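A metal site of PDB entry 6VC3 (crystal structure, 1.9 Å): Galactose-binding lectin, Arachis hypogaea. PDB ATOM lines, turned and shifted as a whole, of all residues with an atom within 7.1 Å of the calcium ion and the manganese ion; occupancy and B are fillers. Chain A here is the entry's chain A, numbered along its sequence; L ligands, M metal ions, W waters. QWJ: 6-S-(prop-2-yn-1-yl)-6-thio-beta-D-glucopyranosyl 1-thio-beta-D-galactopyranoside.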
ATOM      1  N   ASP A  83     -17.757  -9.858  15.053  1.00  0.00           N
ATOM      2  CA  ASP A  83     -18.224  -8.476  15.024  1.00  0.00           C
ATOM      3  C   ASP A  83     -19.617  -8.247  14.449  1.00  0.00           C
ATOM      4  O   ASP A  83     -20.212  -7.180  14.702  1.00  0.00           O
ATOM      5  CB  ASP A  83     -17.205  -7.642  14.253  1.00  0.00           C
ATOM      6  CG  ASP A  83     -16.106  -7.100  15.137  1.00  0.00           C
ATOM      7  OD1 ASP A  83     -15.088  -7.843  15.383  1.00  0.00           O
ATOM      8  OD2 ASP A  83     -16.226  -5.931  15.563  1.00  0.00           O
ATOM      9  N   GLY A  84     -20.131  -9.226  13.711  1.00  0.00           N
ATOM     10  CA  GLY A  84     -21.448  -9.168  13.109  1.00  0.00           C
ATOM     11  C   GLY A  84     -21.477  -9.499  11.644  1.00  0.00           C
ATOM     12  O   GLY A  84     -20.446  -9.818  11.036  1.00  0.00           O
ATOM     13  N   GLY A 103     -12.692  -6.904  11.911  1.00  0.00           N
ATOM     14  CA  GLY A 103     -13.337  -6.271  13.064  1.00  0.00           C
ATOM     15  C   GLY A 103     -14.571  -5.445  12.728  1.00  0.00           C
ATOM     16  O   GLY A 103     -15.539  -5.948  12.144  1.00  0.00           O
ATOM     17  N   GLY A 104     -14.482  -4.163  13.073  1.00  0.00           N
ATOM     18  CA  GLY A 104     -15.544  -3.176  12.901  1.00  0.00           C
ATOM     19  C   GLY A 104     -15.810  -2.767  11.467  1.00  0.00           C
ATOM     20  O   GLY A 104     -16.831  -2.125  11.193  1.00  0.00           O
ATOM     21  N   THR A 105     -14.868  -3.102  10.531  1.00  0.00           N
ATOM     22  CA  THR A 105     -15.030  -2.794   9.105  1.00  0.00           C
ATOM     23  C   THR A 105     -16.152  -3.651   8.501  1.00  0.00           C
ATOM     24  O   THR A 105     -16.658  -3.304   7.442  1.00  0.00           O
ATOM     25  CB  THR A 105     -13.697  -3.001   8.317  1.00  0.00           C
ATOM     26  OG1 THR A 105     -13.355  -4.382   8.257  1.00  0.00           O
ATOM     27  CG2 THR A 105     -12.553  -2.193   8.882  1.00  0.00           C
ATOM     28  N   LEU A 106     -16.484  -4.790   9.152  1.00  0.00           N
ATOM     29  CA  LEU A 106     -17.482  -5.803   8.762  1.00  0.00           C
ATOM     30  C   LEU A 106     -17.137  -6.424   7.381  1.00  0.00           C
ATOM     31  O   LEU A 106     -18.036  -6.942   6.686  1.00  0.00           O
ATOM     32  CB  LEU A 106     -18.933  -5.249   8.795  1.00  0.00           C
ATOM     33  CG  LEU A 106     -19.489  -4.772  10.150  1.00  0.00           C
ATOM     34  CD1 LEU A 106     -20.868  -4.219   9.992  1.00  0.00           C
ATOM     35  CD2 LEU A 106     -19.473  -5.885  11.211  1.00  0.00           C
ATOM     36  N   GLU A 121     -26.483  -3.837   8.240  1.00  0.00           N
ATOM     37  CA  GLU A 121     -25.630  -4.492   9.205  1.00  0.00           C
ATOM     38  C   GLU A 121     -26.409  -4.968  10.442  1.00  0.00           C
ATOM     39  O   GLU A 121     -27.443  -4.388  10.808  1.00  0.00           O
ATOM     40  CB  GLU A 121     -24.475  -3.573   9.638  1.00  0.00           C
ATOM     41  CG  GLU A 121     -24.918  -2.267  10.262  1.00  0.00           C
ATOM     42  CD  GLU A 121     -23.834  -1.553  11.039  1.00  0.00           C
ATOM     43  OE1 GLU A 121     -22.774  -1.274  10.443  1.00  0.00           O
ATOM     44  OE2 GLU A 121     -24.068  -1.229  12.223  1.00  0.00           O
ATOM     45  N   PHE A 122     -25.883  -6.044  11.047  1.00  0.00           N
ATOM     46  CA  PHE A 122     -26.362  -6.703  12.264  1.00  0.00           C
ATOM     47  C   PHE A 122     -25.151  -6.736  13.183  1.00  0.00           C
ATOM     48  O   PHE A 122     -24.429  -7.740  13.286  1.00  0.00           O
ATOM     49  CB  PHE A 122     -26.944  -8.091  11.936  1.00  0.00           C
ATOM     50  CG  PHE A 122     -28.115  -8.022  10.987  1.00  0.00           C
ATOM     51  CD1 PHE A 122     -29.409  -7.875  11.472  1.00  0.00           C
ATOM     52  CD2 PHE A 122     -27.923  -8.058   9.604  1.00  0.00           C
ATOM     53  CE1 PHE A 122     -30.496  -7.796  10.584  1.00  0.00           C
ATOM     54  CE2 PHE A 122     -28.997  -7.953   8.729  1.00  0.00           C
ATOM     55  CZ  PHE A 122     -30.276  -7.816   9.227  1.00  0.00           C
ATOM     56  N   ASP A 123     -24.892  -5.579  13.759  1.00  0.00           N
ATOM     57  CA  ASP A 123     -23.751  -5.258  14.571  1.00  0.00           C
ATOM     58  C   ASP A 123     -23.911  -5.677  16.023  1.00  0.00           C
ATOM     59  O   ASP A 123     -24.865  -5.263  16.689  1.00  0.00           O
ATOM     60  CB  ASP A 123     -23.489  -3.757  14.469  1.00  0.00           C
ATOM     61  CG  ASP A 123     -22.060  -3.383  14.732  1.00  0.00           C
ATOM     62  OD1 ASP A 123     -21.390  -4.101  15.489  1.00  0.00           O
ATOM     63  OD2 ASP A 123     -21.601  -2.395  14.147  1.00  0.00           O
ATOM     64  N   THR A 124     -22.891  -6.462  16.517  1.00  0.00           N
ATOM     65  CA  THR A 124     -22.827  -7.074  17.846  1.00  0.00           C
ATOM     66  C   THR A 124     -21.667  -6.547  18.722  1.00  0.00           C
ATOM     67  O   THR A 124     -21.447  -7.081  19.805  1.00  0.00           O
ATOM     68  CB  THR A 124     -22.675  -8.610  17.695  1.00  0.00           C
ATOM     69  OG1 THR A 124     -21.378  -8.937  17.217  1.00  0.00           O
ATOM     70  CG2 THR A 124     -23.740  -9.213  16.808  1.00  0.00           C
ATOM     71  N   TYR A 125     -20.975  -5.476  18.278  1.00  0.00           N
ATOM     72  CA  TYR A 125     -19.870  -4.850  19.039  1.00  0.00           C
ATOM     73  C   TYR A 125     -19.874  -3.332  18.811  1.00  0.00           C
ATOM     74  O   TYR A 125     -19.992  -2.892  17.665  1.00  0.00           O
ATOM     75  CB  TYR A 125     -18.490  -5.453  18.690  1.00  0.00           C
ATOM     76  CG  TYR A 125     -17.361  -4.868  19.515  1.00  0.00           C
ATOM     77  CD1 TYR A 125     -16.722  -3.692  19.122  1.00  0.00           C
ATOM     78  CD2 TYR A 125     -16.972  -5.449  20.717  1.00  0.00           C
ATOM     79  CE1 TYR A 125     -15.757  -3.088  19.934  1.00  0.00           C
ATOM     80  CE2 TYR A 125     -15.970  -4.883  21.504  1.00  0.00           C
ATOM     81  CZ  TYR A 125     -15.366  -3.697  21.105  1.00  0.00           C
ATOM     82  OH  TYR A 125     -14.374  -3.115  21.868  1.00  0.00           O
ATOM     83  N   SER A 126     -19.685  -2.549  19.895  1.00  0.00           N
ATOM     84  CA  SER A 126     -19.698  -1.095  19.815  1.00  0.00           C
ATOM     85  C   SER A 126     -18.299  -0.523  19.556  1.00  0.00           C
ATOM     86  O   SER A 126     -17.461  -0.436  20.457  1.00  0.00           O
ATOM     87  CB  SER A 126     -20.307  -0.471  21.074  1.00  0.00           C
ATOM     88  OG  SER A 126     -20.540   0.911  20.893  1.00  0.00           O
ATOM     89  N   ASN A 127     -18.072  -0.112  18.299  1.00  0.00           N
ATOM     90  CA  ASN A 127     -16.859   0.511  17.781  1.00  0.00           C
ATOM     91  C   ASN A 127     -16.983   2.035  17.826  1.00  0.00           C
ATOM     92  O   ASN A 127     -17.629   2.616  16.959  1.00  0.00           O
ATOM     93  CB  ASN A 127     -16.573   0.024  16.346  1.00  0.00           C
ATOM     94  CG  ASN A 127     -16.192  -1.430  16.261  1.00  0.00           C
ATOM     95  OD1 ASN A 127     -17.045  -2.300  16.108  1.00  0.00           O
ATOM     96  ND2 ASN A 127     -14.904  -1.718  16.388  1.00  0.00           N
ATOM     97  N   SER A 128     -16.328   2.687  18.824  1.00  0.00           N
ATOM     98  CA  SER A 128     -16.382   4.147  19.001  1.00  0.00           C
ATOM     99  C   SER A 128     -15.792   4.887  17.819  1.00  0.00           C
ATOM    100  O   SER A 128     -16.258   5.978  17.489  1.00  0.00           O
ATOM    101  CB  SER A 128     -15.696   4.569  20.301  1.00  0.00           C
ATOM    102  OG  SER A 128     -14.356   4.114  20.363  1.00  0.00           O
ATOM    103  N   TYR A 130     -16.213   4.225  14.753  1.00  0.00           N
ATOM    104  CA  TYR A 130     -17.232   4.306  13.690  1.00  0.00           C
ATOM    105  C   TYR A 130     -18.560   4.850  14.244  1.00  0.00           C
ATOM    106  O   TYR A 130     -19.602   4.695  13.602  1.00  0.00           O
ATOM    107  CB  TYR A 130     -17.432   2.941  12.997  1.00  0.00           C
ATOM    108  CG  TYR A 130     -16.125   2.301  12.551  1.00  0.00           C
ATOM    109  CD1 TYR A 130     -15.221   2.999  11.760  1.00  0.00           C
ATOM    110  CD2 TYR A 130     -15.815   0.990  12.911  1.00  0.00           C
ATOM    111  CE1 TYR A 130     -14.016   2.422  11.368  1.00  0.00           C
ATOM    112  CE2 TYR A 130     -14.624   0.409  12.509  1.00  0.00           C
ATOM    113  CZ  TYR A 130     -13.727   1.115  11.727  1.00  0.00           C
ATOM    114  OH  TYR A 130     -12.558   0.538  11.324  1.00  0.00           O
ATOM    115  N   ASN A 131     -18.512   5.515  15.419  1.00  0.00           N
ATOM    116  CA  ASN A 131     -19.634   6.111  16.154  1.00  0.00           C
ATOM    117  C   ASN A 131     -20.836   5.148  16.298  1.00  0.00           C
ATOM    118  O   ASN A 131     -21.980   5.523  16.048  1.00  0.00           O
ATOM    119  CB  ASN A 131     -20.059   7.458  15.523  1.00  0.00           C
ATOM    120  CG  ASN A 131     -19.048   8.556  15.688  1.00  0.00           C
ATOM    121  OD1 ASN A 131     -18.590   8.869  16.791  1.00  0.00           O
ATOM    122  ND2 ASN A 131     -18.700   9.191  14.580  1.00  0.00           N
ATOM    123  N   ASP A 132     -20.545   3.903  16.707  1.00  0.00           N
ATOM    124  CA  ASP A 132     -21.555   2.875  16.937  1.00  0.00           C
ATOM    125  C   ASP A 132     -22.449   3.208  18.140  1.00  0.00           C
ATOM    126  O   ASP A 132     -21.925   3.670  19.153  1.00  0.00           O
ATOM    127  CB  ASP A 132     -20.889   1.507  17.212  1.00  0.00           C
ATOM    128  CG  ASP A 132     -20.646   0.619  16.009  1.00  0.00           C
ATOM    129  OD1 ASP A 132     -21.339   0.781  14.989  1.00  0.00           O
ATOM    130  OD2 ASP A 132     -19.820  -0.310  16.121  1.00  0.00           O
ATOM    131  N   PRO A 133     -23.767   2.894  18.123  1.00  0.00           N
ATOM    132  CA  PRO A 133     -24.588   3.107  19.334  1.00  0.00           C
ATOM    133  C   PRO A 133     -24.090   2.203  20.485  1.00  0.00           C
ATOM    134  O   PRO A 133     -23.307   1.281  20.218  1.00  0.00           O
ATOM    135  CB  PRO A 133     -26.012   2.780  18.874  1.00  0.00           C
ATOM    136  CG  PRO A 133     -25.856   1.985  17.651  1.00  0.00           C
ATOM    137  CD  PRO A 133     -24.573   2.343  17.010  1.00  0.00           C
ATOM    138  N   THR A 135     -25.389  -0.291  22.338  1.00  0.00           N
ATOM    139  CA  THR A 135     -25.828  -1.692  22.372  1.00  0.00           C
ATOM    140  C   THR A 135     -25.826  -2.326  20.975  1.00  0.00           C
ATOM    141  O   THR A 135     -25.613  -1.604  19.987  1.00  0.00           O
ATOM    142  CB  THR A 135     -27.246  -1.799  22.977  1.00  0.00           C
ATOM    143  OG1 THR A 135     -28.203  -1.204  22.100  1.00  0.00           O
ATOM    144  CG2 THR A 135     -27.350  -1.200  24.378  1.00  0.00           C
ATOM    145  N   HIS A 137     -27.148  -3.609  17.409  1.00  0.00           N
ATOM    146  CA  HIS A 137     -28.040  -2.851  16.538  1.00  0.00           C
ATOM    147  C   HIS A 137     -28.110  -3.318  15.113  1.00  0.00           C
ATOM    148  O   HIS A 137     -27.224  -3.977  14.577  1.00  0.00           O
ATOM    149  CB  HIS A 137     -27.635  -1.358  16.513  1.00  0.00           C
ATOM    150  CG  HIS A 137     -26.193  -1.135  16.161  1.00  0.00           C
ATOM    151  ND1 HIS A 137     -25.200  -1.281  17.103  1.00  0.00           N
ATOM    152  CD2 HIS A 137     -25.630  -0.802  14.977  1.00  0.00           C
ATOM    153  CE1 HIS A 137     -24.076  -0.993  16.477  1.00  0.00           C
ATOM    154  NE2 HIS A 137     -24.292  -0.697  15.201  1.00  0.00           N
ATOM    155  N   VAL A 138     -29.208  -2.895  14.477  1.00  0.00           N
ATOM    156  CA  VAL A 138     -29.412  -3.066  13.057  1.00  0.00           C
ATOM    157  C   VAL A 138     -29.141  -1.677  12.491  1.00  0.00           C
ATOM    158  O   VAL A 138     -29.562  -0.687  13.090  1.00  0.00           O
ATOM    159  CB  VAL A 138     -30.793  -3.663  12.706  1.00  0.00           C
ATOM    160  CG1 VAL A 138     -30.968  -3.792  11.190  1.00  0.00           C
ATOM    161  CG2 VAL A 138     -30.969  -5.018  13.371  1.00  0.00           C
ATOM    162  N   GLY A 139     -28.321  -1.597  11.458  1.00  0.00           N
ATOM    163  CA  GLY A 139     -27.933  -0.328  10.870  1.00  0.00           C
ATOM    164  C   GLY A 139     -28.060  -0.331   9.367  1.00  0.00           C
ATOM    165  O   GLY A 139     -27.988  -1.377   8.725  1.00  0.00           O
ATOM    166  N   ASP A 141     -26.360   1.354   6.102  1.00  0.00           N
ATOM    167  CA  ASP A 141     -25.026   1.849   5.730  1.00  0.00           C
ATOM    168  C   ASP A 141     -24.959   2.309   4.291  1.00  0.00           C
ATOM    169  O   ASP A 141     -25.439   1.608   3.394  1.00  0.00           O
ATOM    170  CB  ASP A 141     -23.994   0.714   5.943  1.00  0.00           C
ATOM    171  CG  ASP A 141     -23.737   0.335   7.387  1.00  0.00           C
ATOM    172  OD1 ASP A 141     -24.463   0.865   8.279  1.00  0.00           O
ATOM    173  OD2 ASP A 141     -22.796  -0.483   7.640  1.00  0.00           O
ATOM    174  N   VAL A 145     -19.350   2.274   7.469  1.00  0.00           N
ATOM    175  CA  VAL A 145     -19.804   1.463   8.603  1.00  0.00           C
ATOM    176  C   VAL A 145     -20.230   2.423   9.746  1.00  0.00           C
ATOM    177  O   VAL A 145     -20.678   1.991  10.812  1.00  0.00           O
ATOM    178  CB  VAL A 145     -18.834   0.346   9.075  1.00  0.00           C
ATOM    179  CG1 VAL A 145     -18.807  -0.817   8.089  1.00  0.00           C
ATOM    180  CG2 VAL A 145     -17.423   0.871   9.344  1.00  0.00           C
ATOM    181  N   ASP A 146     -20.094   3.734   9.519  1.00  0.00           N
ATOM    182  CA  ASP A 146     -20.658   4.770  10.389  1.00  0.00           C
ATOM    183  C   ASP A 146     -22.054   4.973   9.799  1.00  0.00           C
ATOM    184  O   ASP A 146     -22.219   5.705   8.823  1.00  0.00           O
ATOM    185  CB  ASP A 146     -19.786   6.057  10.428  1.00  0.00           C
ATOM    186  CG  ASP A 146     -20.204   7.109  11.454  1.00  0.00           C
ATOM    187  OD1 ASP A 146     -21.360   7.063  11.937  1.00  0.00           O
ATOM    188  OD2 ASP A 146     -19.383   7.994  11.766  1.00  0.00           O
ATOM    189  N   SER A 147     -23.028   4.184  10.307  1.00  0.00           N
ATOM    190  CA  SER A 147     -24.401   4.076   9.819  1.00  0.00           C
ATOM    191  C   SER A 147     -25.127   5.406   9.642  1.00  0.00           C
ATOM    192  O   SER A 147     -25.006   6.317  10.485  1.00  0.00           O
ATOM    193  CB  SER A 147     -25.239   3.197  10.743  1.00  0.00           C
ATOM    194  OG  SER A 147     -24.859   1.825  10.736  1.00  0.00           O
ATOM    195  N   THR A 150     -29.505   3.815  12.756  1.00  0.00           N
ATOM    196  CA  THR A 150     -29.459   2.581  13.540  1.00  0.00           C
ATOM    197  C   THR A 150     -30.722   2.413  14.371  1.00  0.00           C
ATOM    198  O   THR A 150     -31.381   3.386  14.699  1.00  0.00           O
ATOM    199  CB  THR A 150     -28.234   2.514  14.494  1.00  0.00           C
ATOM    200  OG1 THR A 150     -28.254   3.638  15.366  1.00  0.00           O
ATOM    201  CG2 THR A 150     -26.907   2.369  13.762  1.00  0.00           C
HETATM  202  C4  QWJ L   1     -13.831  -5.829  18.109  1.00  0.00           C
HETATM  203  C3  QWJ L   1     -13.451  -4.533  17.379  1.00  0.00           C
HETATM  204  C5  QWJ L   1     -13.065  -5.918  19.423  1.00  0.00           C
HETATM  205  C1  QWJ L   1     -11.256  -4.608  18.574  1.00  0.00           C
HETATM  206  C2  QWJ L   1     -11.936  -4.435  17.219  1.00  0.00           C
HETATM  207  C6  QWJ L   1     -13.307  -7.195  20.189  1.00  0.00           C
HETATM  208  O5  QWJ L   1     -11.651  -5.838  19.178  1.00  0.00           O
HETATM  209  O2  QWJ L   1     -11.577  -3.198  16.633  1.00  0.00           O
HETATM  210  O3  QWJ L   1     -14.093  -4.467  16.115  1.00  0.00           O
HETATM  211  O4  QWJ L   1     -13.504  -6.950  17.299  1.00  0.00           O
HETATM  212  O6  QWJ L   1     -13.197  -6.999  21.586  1.00  0.00           O
HETATM  213  S1  QWJ L   1      -9.460  -4.511  18.432  1.00  0.00           S
HETATM  214 CA    CA M   1     -19.380  -2.505  15.572  1.00  0.00          CA
HETATM  215 MN    MN M   2     -22.537  -0.566  13.847  1.00  0.00          MN
HETATM  216  O   HOH W   1     -21.167  -0.252  12.295  1.00  0.00           O
HETATM  217  O   HOH W   2     -18.449  -4.505  14.977  1.00  0.00           O
HETATM  218  O   HOH W   3     -18.774  -1.812  13.518  1.00  0.00           O
HETATM  219  O   HOH W   4     -23.695   1.282  13.331  1.00  0.00           O
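ND2 of Asn 127 is in hydrogen-bond range of O3 of the ligand. An oxygen (O4) of the ligand lies within hydrogen-bond range of the side-chain carboxylate (OD1) of Asp 83 (2.6 Å). O3 of the ligand lies within hydrogen-bond range of N of Gly 104.
The backbone carbonyl oxygen of Gly 139 lies within hydrogen-bond range of the backbone NH of Glu 121 (2.9 Å). The side-chain carboxylate of Glu 121 lies close to the side-chain hydroxyl of Ser 147, at 3.5 Å. A ring nitrogen (ND1) of His 137 sits at hydrogen-bond distance from the backbone carbonyl oxygen (O) of Thr 135 (2.9 Å).
Of the 27 residues printed, 4 come within 4 Å of the calcium ion. The nearest printed residue that does not touch the calcium ion is Ser 126 (4.3 Å).
Of the 27 residues printed, 4 come within 4 Å of the manganese ion.
The calcium ion is bound by the backbone carbonyl oxygen (O) of Tyr 125 (2.2 Å), water W3 (2.3 Å), water W2 (2.3 Å), the side-chain carboxylate (OD2) of Asp 132 (2.3 Å), the side-chain amide oxygen (OD1) of Asn 127 (2.4 Å), the side-chain carboxylate (OD1) of Asp 123 (2.6 Å) and the side-chain carboxylate (OD2) of Asp 123 (2.6 Å). The calcium ion has seven donor atoms within binding distance.
The manganese ion is bound by the side-chain carboxylate (OD2) of Asp 123 (2.1 Å). Water W1 binds the manganese ion (2.1 Å). OD1 of Asp 132 binds the manganese ion (2.1 Å). NE2 of His 137 binds the manganese ion, at 2.2 Å. The manganese ion is bound by water W4 (2.2 Å). The manganese ion is bound by OE2 of Glu 121 (2.3 Å).
Water W1 bridges OE1 of Glu 121 (2.7 Å) and O of Val 145 (2.7 Å).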
